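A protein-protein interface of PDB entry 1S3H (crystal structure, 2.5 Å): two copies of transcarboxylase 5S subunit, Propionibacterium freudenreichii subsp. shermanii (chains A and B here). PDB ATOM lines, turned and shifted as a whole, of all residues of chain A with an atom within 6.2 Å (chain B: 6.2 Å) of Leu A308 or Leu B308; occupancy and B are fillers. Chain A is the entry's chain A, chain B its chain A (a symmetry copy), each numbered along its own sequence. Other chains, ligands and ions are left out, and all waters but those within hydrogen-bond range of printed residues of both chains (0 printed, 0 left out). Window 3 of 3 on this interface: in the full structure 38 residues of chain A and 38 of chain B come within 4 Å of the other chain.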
ATOM      1  N   SER A 229     -11.746  31.802  -9.292  1.00  0.00           N
ATOM      2  CA  SER A 229     -10.383  31.327  -9.567  1.00  0.00           C
ATOM      3  C   SER A 229      -9.732  32.193 -10.646  1.00  0.00           C
ATOM      4  O   SER A 229      -8.664  31.860 -11.157  1.00  0.00           O
ATOM      5  CB  SER A 229     -10.436  29.874 -10.048  1.00  0.00           C
ATOM      6  OG  SER A 229     -11.303  29.747 -11.171  1.00  0.00           O
ATOM      7  N   THR A 230     -10.384  33.308 -10.951  1.00  0.00           N
ATOM      8  CA  THR A 230      -9.961  34.242 -12.006  1.00  0.00           C
ATOM      9  C   THR A 230      -8.460  34.541 -11.996  1.00  0.00           C
ATOM     10  O   THR A 230      -7.850  34.604 -13.062  1.00  0.00           O
ATOM     11  CB  THR A 230     -10.738  35.564 -11.906  1.00  0.00           C
ATOM     12  OG1 THR A 230     -12.138  35.274 -11.858  1.00  0.00           O
ATOM     13  CG2 THR A 230     -10.462  36.451 -13.124  1.00  0.00           C
ATOM     14  N   THR A 231      -7.852  34.729 -10.823  1.00  0.00           N
ATOM     15  CA  THR A 231      -6.424  35.072 -10.737  1.00  0.00           C
ATOM     16  C   THR A 231      -5.555  33.842 -10.470  1.00  0.00           C
ATOM     17  O   THR A 231      -4.330  33.910 -10.566  1.00  0.00           O
ATOM     18  CB  THR A 231      -6.151  36.044  -9.608  1.00  0.00           C
ATOM     19  OG1 THR A 231      -6.535  35.434  -8.370  1.00  0.00           O
ATOM     20  CG2 THR A 231      -6.914  37.324  -9.826  1.00  0.00           C
ATOM     21  N   GLY A 232      -6.176  32.739 -10.076  1.00  0.00           N
ATOM     22  CA  GLY A 232      -5.427  31.515  -9.844  1.00  0.00           C
ATOM     23  C   GLY A 232      -4.758  31.310  -8.508  1.00  0.00           C
ATOM     24  O   GLY A 232      -4.019  30.337  -8.367  1.00  0.00           O
ATOM     25  N   SER A 254     -15.706  20.066 -10.820  1.00  0.00           N
ATOM     26  CA  SER A 254     -14.520  20.139 -11.688  1.00  0.00           C
ATOM     27  C   SER A 254     -14.808  20.332 -13.179  1.00  0.00           C
ATOM     28  O   SER A 254     -14.078  21.066 -13.845  1.00  0.00           O
ATOM     29  CB  SER A 254     -13.636  18.904 -11.498  1.00  0.00           C
ATOM     30  OG  SER A 254     -14.345  17.711 -11.795  1.00  0.00           O
ATOM     31  N   SER A 257     -15.295  24.364 -13.747  1.00  0.00           N
ATOM     32  CA  SER A 257     -14.511  25.208 -12.835  1.00  0.00           C
ATOM     33  C   SER A 257     -13.338  25.910 -13.523  1.00  0.00           C
ATOM     34  O   SER A 257     -13.049  25.700 -14.700  1.00  0.00           O
ATOM     35  CB  SER A 257     -13.961  24.321 -11.729  1.00  0.00           C
ATOM     36  OG  SER A 257     -13.250  23.228 -12.302  1.00  0.00           O
ATOM     37  N   LEU A 258     -12.661  26.731 -12.719  1.00  0.00           N
ATOM     38  CA  LEU A 258     -11.463  27.499 -13.089  1.00  0.00           C
ATOM     39  C   LEU A 258     -11.839  28.669 -13.998  1.00  0.00           C
ATOM     40  O   LEU A 258     -13.016  29.002 -14.139  1.00  0.00           O
ATOM     41  CB  LEU A 258     -10.414  26.579 -13.736  1.00  0.00           C
ATOM     42  CG  LEU A 258     -10.008  25.434 -12.794  1.00  0.00           C
ATOM     43  CD1 LEU A 258      -8.953  24.535 -13.419  1.00  0.00           C
ATOM     44  CD2 LEU A 258      -9.475  26.016 -11.525  1.00  0.00           C
ATOM     45  N   GLY A 259     -10.851  29.296 -14.612  1.00  0.00           N
ATOM     46  CA  GLY A 259     -11.175  30.444 -15.429  1.00  0.00           C
ATOM     47  C   GLY A 259     -11.872  31.423 -14.495  1.00  0.00           C
ATOM     48  O   GLY A 259     -11.532  31.477 -13.315  1.00  0.00           O
ATOM     49  N   PRO A 260     -12.842  32.209 -14.981  1.00  0.00           N
ATOM     50  CA  PRO A 260     -13.569  33.181 -14.159  1.00  0.00           C
ATOM     51  C   PRO A 260     -14.554  32.447 -13.247  1.00  0.00           C
ATOM     52  O   PRO A 260     -15.367  33.058 -12.554  1.00  0.00           O
ATOM     53  CB  PRO A 260     -14.292  34.043 -15.194  1.00  0.00           C
ATOM     54  CG  PRO A 260     -13.463  33.881 -16.420  1.00  0.00           C
ATOM     55  CD  PRO A 260     -13.142  32.418 -16.404  1.00  0.00           C
ATOM     56  N   ARG A 297     -21.368  20.497 -21.207  1.00  0.00           N
ATOM     57  CA  ARG A 297     -20.635  21.757 -21.393  1.00  0.00           C
ATOM     58  C   ARG A 297     -20.261  22.073 -22.844  1.00  0.00           C
ATOM     59  O   ARG A 297     -20.463  23.196 -23.303  1.00  0.00           O
ATOM     60  CB  ARG A 297     -19.396  21.804 -20.506  1.00  0.00           C
ATOM     61  CG  ARG A 297     -18.704  23.147 -20.565  1.00  0.00           C
ATOM     62  CD  ARG A 297     -17.603  23.213 -19.571  1.00  0.00           C
ATOM     63  NE  ARG A 297     -16.918  24.497 -19.599  1.00  0.00           N
ATOM     64  CZ  ARG A 297     -15.980  24.861 -18.722  1.00  0.00           C
ATOM     65  NH1 ARG A 297     -15.623  24.037 -17.748  1.00  0.00           N
ATOM     66  NH2 ARG A 297     -15.390  26.041 -18.831  1.00  0.00           N
ATOM     67  N   LYS A 306     -12.019  33.230 -22.842  1.00  0.00           N
ATOM     68  CA  LYS A 306     -10.799  32.607 -23.373  1.00  0.00           C
ATOM     69  C   LYS A 306      -9.550  32.913 -22.544  1.00  0.00           C
ATOM     70  O   LYS A 306      -8.440  32.918 -23.074  1.00  0.00           O
ATOM     71  CB  LYS A 306     -10.639  33.016 -24.834  1.00  0.00           C
ATOM     72  CG  LYS A 306     -11.745  32.404 -25.692  1.00  0.00           C
ATOM     73  CD  LYS A 306     -11.698  32.866 -27.138  1.00  0.00           C
ATOM     74  CE  LYS A 306     -12.010  34.356 -27.259  1.00  0.00           C
ATOM     75  NZ  LYS A 306     -13.469  34.640 -27.086  1.00  0.00           N
ATOM     76  N   THR A 307      -9.729  33.144 -21.243  1.00  0.00           N
ATOM     77  CA  THR A 307      -8.592  33.391 -20.344  1.00  0.00           C
ATOM     78  C   THR A 307      -8.799  32.568 -19.070  1.00  0.00           C
ATOM     79  O   THR A 307      -9.762  32.780 -18.334  1.00  0.00           O
ATOM     80  CB  THR A 307      -8.448  34.905 -19.972  1.00  0.00           C
ATOM     81  OG1 THR A 307      -8.418  35.708 -21.166  1.00  0.00           O
ATOM     82  CG2 THR A 307      -7.141  35.141 -19.205  1.00  0.00           C
ATOM     83  N   LEU A 308      -7.906  31.610 -18.833  1.00  0.00           N
ATOM     84  CA  LEU A 308      -7.997  30.738 -17.653  1.00  0.00           C
ATOM     85  C   LEU A 308      -7.387  31.413 -16.422  1.00  0.00           C
ATOM     86  O   LEU A 308      -7.888  31.256 -15.310  1.00  0.00           O
ATOM     87  CB  LEU A 308      -7.269  29.409 -17.873  1.00  0.00           C
ATOM     88  CG  LEU A 308      -7.933  28.258 -18.633  1.00  0.00           C
ATOM     89  CD1 LEU A 308      -7.168  26.970 -18.297  1.00  0.00           C
ATOM     90  CD2 LEU A 308      -9.396  28.105 -18.232  1.00  0.00           C
ATOM     91  N   VAL A 309      -6.301  32.149 -16.597  1.00  0.00           N
ATOM     92  CA  VAL A 309      -5.674  32.800 -15.438  1.00  0.00           C
ATOM     93  C   VAL A 309      -5.284  34.230 -15.814  1.00  0.00           C
ATOM     94  O   VAL A 309      -4.772  34.476 -16.904  1.00  0.00           O
ATOM     95  CB  VAL A 309      -4.403  32.046 -14.998  1.00  0.00           C
ATOM     96  CG1 VAL A 309      -3.782  32.727 -13.789  1.00  0.00           C
ATOM     97  CG2 VAL A 309      -4.742  30.610 -14.681  1.00  0.00           C
ATOM     98  N   ASP A 310      -5.525  35.159 -14.900  1.00  0.00           N
ATOM     99  CA  ASP A 310      -5.182  36.570 -15.129  1.00  0.00           C
ATOM    100  C   ASP A 310      -4.948  37.244 -13.775  1.00  0.00           C
ATOM    101  O   ASP A 310      -5.861  37.366 -12.960  1.00  0.00           O
ATOM    102  CB  ASP A 310      -6.320  37.259 -15.886  1.00  0.00           C
ATOM    103  CG  ASP A 310      -5.982  38.684 -16.284  1.00  0.00           C
ATOM    104  OD1 ASP A 310      -4.863  39.148 -15.961  1.00  0.00           O
ATOM    105  OD2 ASP A 310      -6.836  39.342 -16.919  1.00  0.00           O
ATOM    106  N   SER B 229      -0.714  20.229 -12.756  1.00  0.00           N
ATOM    107  CA  SER B 229      -1.969  20.712 -12.162  1.00  0.00           C
ATOM    108  C   SER B 229      -3.129  19.807 -12.577  1.00  0.00           C
ATOM    109  O   SER B 229      -4.292  20.133 -12.343  1.00  0.00           O
ATOM    110  CB  SER B 229      -2.243  22.141 -12.643  1.00  0.00           C
ATOM    111  OG  SER B 229      -2.246  22.201 -14.066  1.00  0.00           O
ATOM    112  N   THR B 230      -2.782  18.669 -13.164  1.00  0.00           N
ATOM    113  CA  THR B 230      -3.746  17.694 -13.696  1.00  0.00           C
ATOM    114  C   THR B 230      -4.923  17.419 -12.757  1.00  0.00           C
ATOM    115  O   THR B 230      -6.056  17.316 -13.223  1.00  0.00           O
ATOM    116  CB  THR B 230      -3.049  16.366 -14.030  1.00  0.00           C
ATOM    117  OG1 THR B 230      -1.917  16.635 -14.861  1.00  0.00           O
ATOM    118  CG2 THR B 230      -3.998  15.427 -14.783  1.00  0.00           C
ATOM    119  N   THR B 231      -4.685  17.296 -11.449  1.00  0.00           N
ATOM    120  CA  THR B 231      -5.757  16.980 -10.493  1.00  0.00           C
ATOM    121  C   THR B 231      -6.301  18.235  -9.808  1.00  0.00           C
ATOM    122  O   THR B 231      -7.329  18.182  -9.132  1.00  0.00           O
ATOM    123  CB  THR B 231      -5.268  16.067  -9.389  1.00  0.00           C
ATOM    124  OG1 THR B 231      -4.217  16.728  -8.674  1.00  0.00           O
ATOM    125  CG2 THR B 231      -4.777  14.766  -9.967  1.00  0.00           C
ATOM    126  N   GLY B 232      -5.587  19.345  -9.928  1.00  0.00           N
ATOM    127  CA  GLY B 232      -6.057  20.590  -9.344  1.00  0.00           C
ATOM    128  C   GLY B 232      -5.773  20.868  -7.889  1.00  0.00           C
ATOM    129  O   GLY B 232      -6.287  21.858  -7.372  1.00  0.00           O
ATOM    130  N   SER B 254       1.298  31.816 -16.932  1.00  0.00           N
ATOM    131  CA  SER B 254      -0.169  31.722 -16.889  1.00  0.00           C
ATOM    132  C   SER B 254      -0.849  31.454 -18.234  1.00  0.00           C
ATOM    133  O   SER B 254      -1.822  30.702 -18.280  1.00  0.00           O
ATOM    134  CB  SER B 254      -0.772  32.978 -16.256  1.00  0.00           C
ATOM    135  OG  SER B 254      -0.412  34.145 -16.980  1.00  0.00           O
ATOM    136  N   SER B 257      -0.747  27.393 -18.792  1.00  0.00           N
ATOM    137  CA  SER B 257      -0.796  26.605 -17.553  1.00  0.00           C
ATOM    138  C   SER B 257      -2.134  25.891 -17.347  1.00  0.00           C
ATOM    139  O   SER B 257      -3.085  26.051 -18.110  1.00  0.00           O
ATOM    140  CB  SER B 257      -0.570  27.552 -16.385  1.00  0.00           C
ATOM    141  OG  SER B 257      -1.500  28.628 -16.454  1.00  0.00           O
ATOM    142  N   LEU B 258      -2.165  25.120 -16.259  1.00  0.00           N
ATOM    143  CA  LEU B 258      -3.327  24.354 -15.785  1.00  0.00           C
ATOM    144  C   LEU B 258      -3.566  23.137 -16.678  1.00  0.00           C
ATOM    145  O   LEU B 258      -2.716  22.779 -17.492  1.00  0.00           O
ATOM    146  CB  LEU B 258      -4.567  25.259 -15.698  1.00  0.00           C
ATOM    147  CG  LEU B 258      -4.331  26.453 -14.758  1.00  0.00           C
ATOM    148  CD1 LEU B 258      -5.562  27.339 -14.649  1.00  0.00           C
ATOM    149  CD2 LEU B 258      -3.968  25.940 -13.402  1.00  0.00           C
ATOM    150  N   GLY B 259      -4.714  22.497 -16.529  1.00  0.00           N
ATOM    151  CA  GLY B 259      -4.938  21.307 -17.320  1.00  0.00           C
ATOM    152  C   GLY B 259      -3.800  20.362 -16.962  1.00  0.00           C
ATOM    153  O   GLY B 259      -3.347  20.369 -15.819  1.00  0.00           O
ATOM    154  N   PRO B 260      -3.318  19.539 -17.902  1.00  0.00           N
ATOM    155  CA  PRO B 260      -2.223  18.595 -17.652  1.00  0.00           C
ATOM    156  C   PRO B 260      -0.898  19.355 -17.567  1.00  0.00           C
ATOM    157  O   PRO B 260       0.178  18.765 -17.488  1.00  0.00           O
ATOM    158  CB  PRO B 260      -2.270  17.674 -18.871  1.00  0.00           C
ATOM    159  CG  PRO B 260      -3.678  17.792 -19.341  1.00  0.00           C
ATOM    160  CD  PRO B 260      -3.946  19.259 -19.200  1.00  0.00           C
ATOM    161  N   ARG B 297      -0.561  30.811 -28.579  1.00  0.00           N
ATOM    162  CA  ARG B 297      -1.235  29.555 -28.219  1.00  0.00           C
ATOM    163  C   ARG B 297      -2.412  29.177 -29.122  1.00  0.00           C
ATOM    164  O   ARG B 297      -2.515  28.031 -29.556  1.00  0.00           O
ATOM    165  CB  ARG B 297      -1.673  29.569 -26.759  1.00  0.00           C
ATOM    166  CG  ARG B 297      -2.235  28.236 -26.320  1.00  0.00           C
ATOM    167  CD  ARG B 297      -2.498  28.234 -24.858  1.00  0.00           C
ATOM    168  NE  ARG B 297      -3.036  26.962 -24.402  1.00  0.00           N
ATOM    169  CZ  ARG B 297      -3.237  26.654 -23.119  1.00  0.00           C
ATOM    170  NH1 ARG B 297      -2.937  27.528 -22.169  1.00  0.00           N
ATOM    171  NH2 ARG B 297      -3.752  25.480 -22.789  1.00  0.00           N
ATOM    172  N   LYS B 306      -8.756  18.165 -23.563  1.00  0.00           N
ATOM    173  CA  LYS B 306     -10.056  18.783 -23.266  1.00  0.00           C
ATOM    174  C   LYS B 306     -10.533  18.536 -21.833  1.00  0.00           C
ATOM    175  O   LYS B 306     -11.735  18.523 -21.574  1.00  0.00           O
ATOM    176  CB  LYS B 306     -11.069  18.308 -24.304  1.00  0.00           C
ATOM    177  CG  LYS B 306     -10.728  18.861 -25.686  1.00  0.00           C
ATOM    178  CD  LYS B 306     -11.642  18.334 -26.778  1.00  0.00           C
ATOM    179  CE  LYS B 306     -11.444  16.835 -26.995  1.00  0.00           C
ATOM    180  NZ  LYS B 306     -10.180  16.536 -27.737  1.00  0.00           N
ATOM    181  N   THR B 307      -9.592  18.363 -20.904  1.00  0.00           N
ATOM    182  CA  THR B 307      -9.940  18.176 -19.487  1.00  0.00           C
ATOM    183  C   THR B 307      -9.010  19.054 -18.646  1.00  0.00           C
ATOM    184  O   THR B 307      -7.794  18.862 -18.642  1.00  0.00           O
ATOM    185  CB  THR B 307      -9.802  16.684 -19.034  1.00  0.00           C
ATOM    186  OG1 THR B 307     -10.542  15.826 -19.922  1.00  0.00           O
ATOM    187  CG2 THR B 307     -10.363  16.505 -17.618  1.00  0.00           C
ATOM    188  N   LEU B 308      -9.587  20.036 -17.957  1.00  0.00           N
ATOM    189  CA  LEU B 308      -8.808  20.961 -17.121  1.00  0.00           C
ATOM    190  C   LEU B 308      -8.527  20.354 -15.744  1.00  0.00           C
ATOM    191  O   LEU B 308      -7.454  20.555 -15.180  1.00  0.00           O
ATOM    192  CB  LEU B 308      -9.540  22.289 -16.912  1.00  0.00           C
ATOM    193  CG  LEU B 308      -9.497  23.393 -17.972  1.00  0.00           C
ATOM    194  CD1 LEU B 308      -9.917  24.707 -17.300  1.00  0.00           C
ATOM    195  CD2 LEU B 308      -8.096  23.541 -18.557  1.00  0.00           C
ATOM    196  N   VAL B 309      -9.482  19.628 -15.185  1.00  0.00           N
ATOM    197  CA  VAL B 309      -9.259  19.042 -13.856  1.00  0.00           C
ATOM    198  C   VAL B 309      -9.775  17.603 -13.847  1.00  0.00           C
ATOM    199  O   VAL B 309     -10.843  17.313 -14.384  1.00  0.00           O
ATOM    200  CB  VAL B 309     -10.009  19.836 -12.766  1.00  0.00           C
ATOM    201  CG1 VAL B 309      -9.750  19.222 -11.399  1.00  0.00           C
ATOM    202  CG2 VAL B 309      -9.570  21.279 -12.789  1.00  0.00           C
ATOM    203  N   ASP B 310      -9.011  16.713 -13.229  1.00  0.00           N
ATOM    204  CA  ASP B 310      -9.399  15.298 -13.134  1.00  0.00           C
ATOM    205  C   ASP B 310      -8.747  14.692 -11.890  1.00  0.00           C
ATOM    206  O   ASP B 310      -7.525  14.595 -11.798  1.00  0.00           O
ATOM    207  CB  ASP B 310      -8.951  14.557 -14.396  1.00  0.00           C
ATOM    208  CG  ASP B 310      -9.439  13.121 -14.437  1.00  0.00           C
ATOM    209  OD1 ASP B 310     -10.120  12.690 -13.477  1.00  0.00           O
ATOM    210  OD2 ASP B 310      -9.141  12.420 -15.431  1.00  0.00           O
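The backbone carbonyl oxygen (O) of Ser B254 is in hydrogen-bond range of the side-chain hydroxyl (OG) of Ser B257 (2.8 Å). O of Ser A254 sits at hydrogen-bond distance from OG of Ser A257, 2.8 Å away.
Printed residues of chain B within 4 Å of Leu A258: Val B309. Of the printed residues of chain B, Leu A308 touches Leu B308 (3.6 Å). Of the printed residues of chain B, Val A309 touches Ser B254 (3.9 Å) and Leu B258 (3.4 Å). Ser B229 touches none of the printed residues of chain A. Of the printed residues of chain A, Ser B254 touches Val A309 (3.9 Å). Of the printed residues of chain A, Leu B308 touches Leu A308. Of the printed residues of chain A, Val B309 touches Ser A254 (3.9 Å) and Leu A258 (3.4 Å).
Ser A254 touches Val B309, and with the chains exchanged Val A309 touches Ser B254. Leu A258 touches Val B309, and with the chains exchanged Val A309 touches Leu B258. Leu A308 touches its own counterpart, Leu B308. Of the 5 pairs that touch across the chains among the printed residues, 5 have their exchanged pair printed and touching as well.
Of the 15 printed residues of chain B, 4 touch a printed residue of chain A. Of the 15 printed residues of chain A, 4 touch a printed residue of chain B. Printed residues of chain A that touch a printed residue of chain B: Ser A254, Leu A258, Leu A308 and Val A309. Hydrophobic or aromatic side chains of chain A that line the printed part of chain B: Leu A258, Leu A308 and Val A309. Among the printed residues, 5 pairs touch across the chains.
Among the printed residues, merely in contact across the chains: Val A309 with Leu B258, Leu A258 with Val B309, Leu A308 with Leu B308, Val A309 with Ser B254 and Ser A254 with Val B309.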
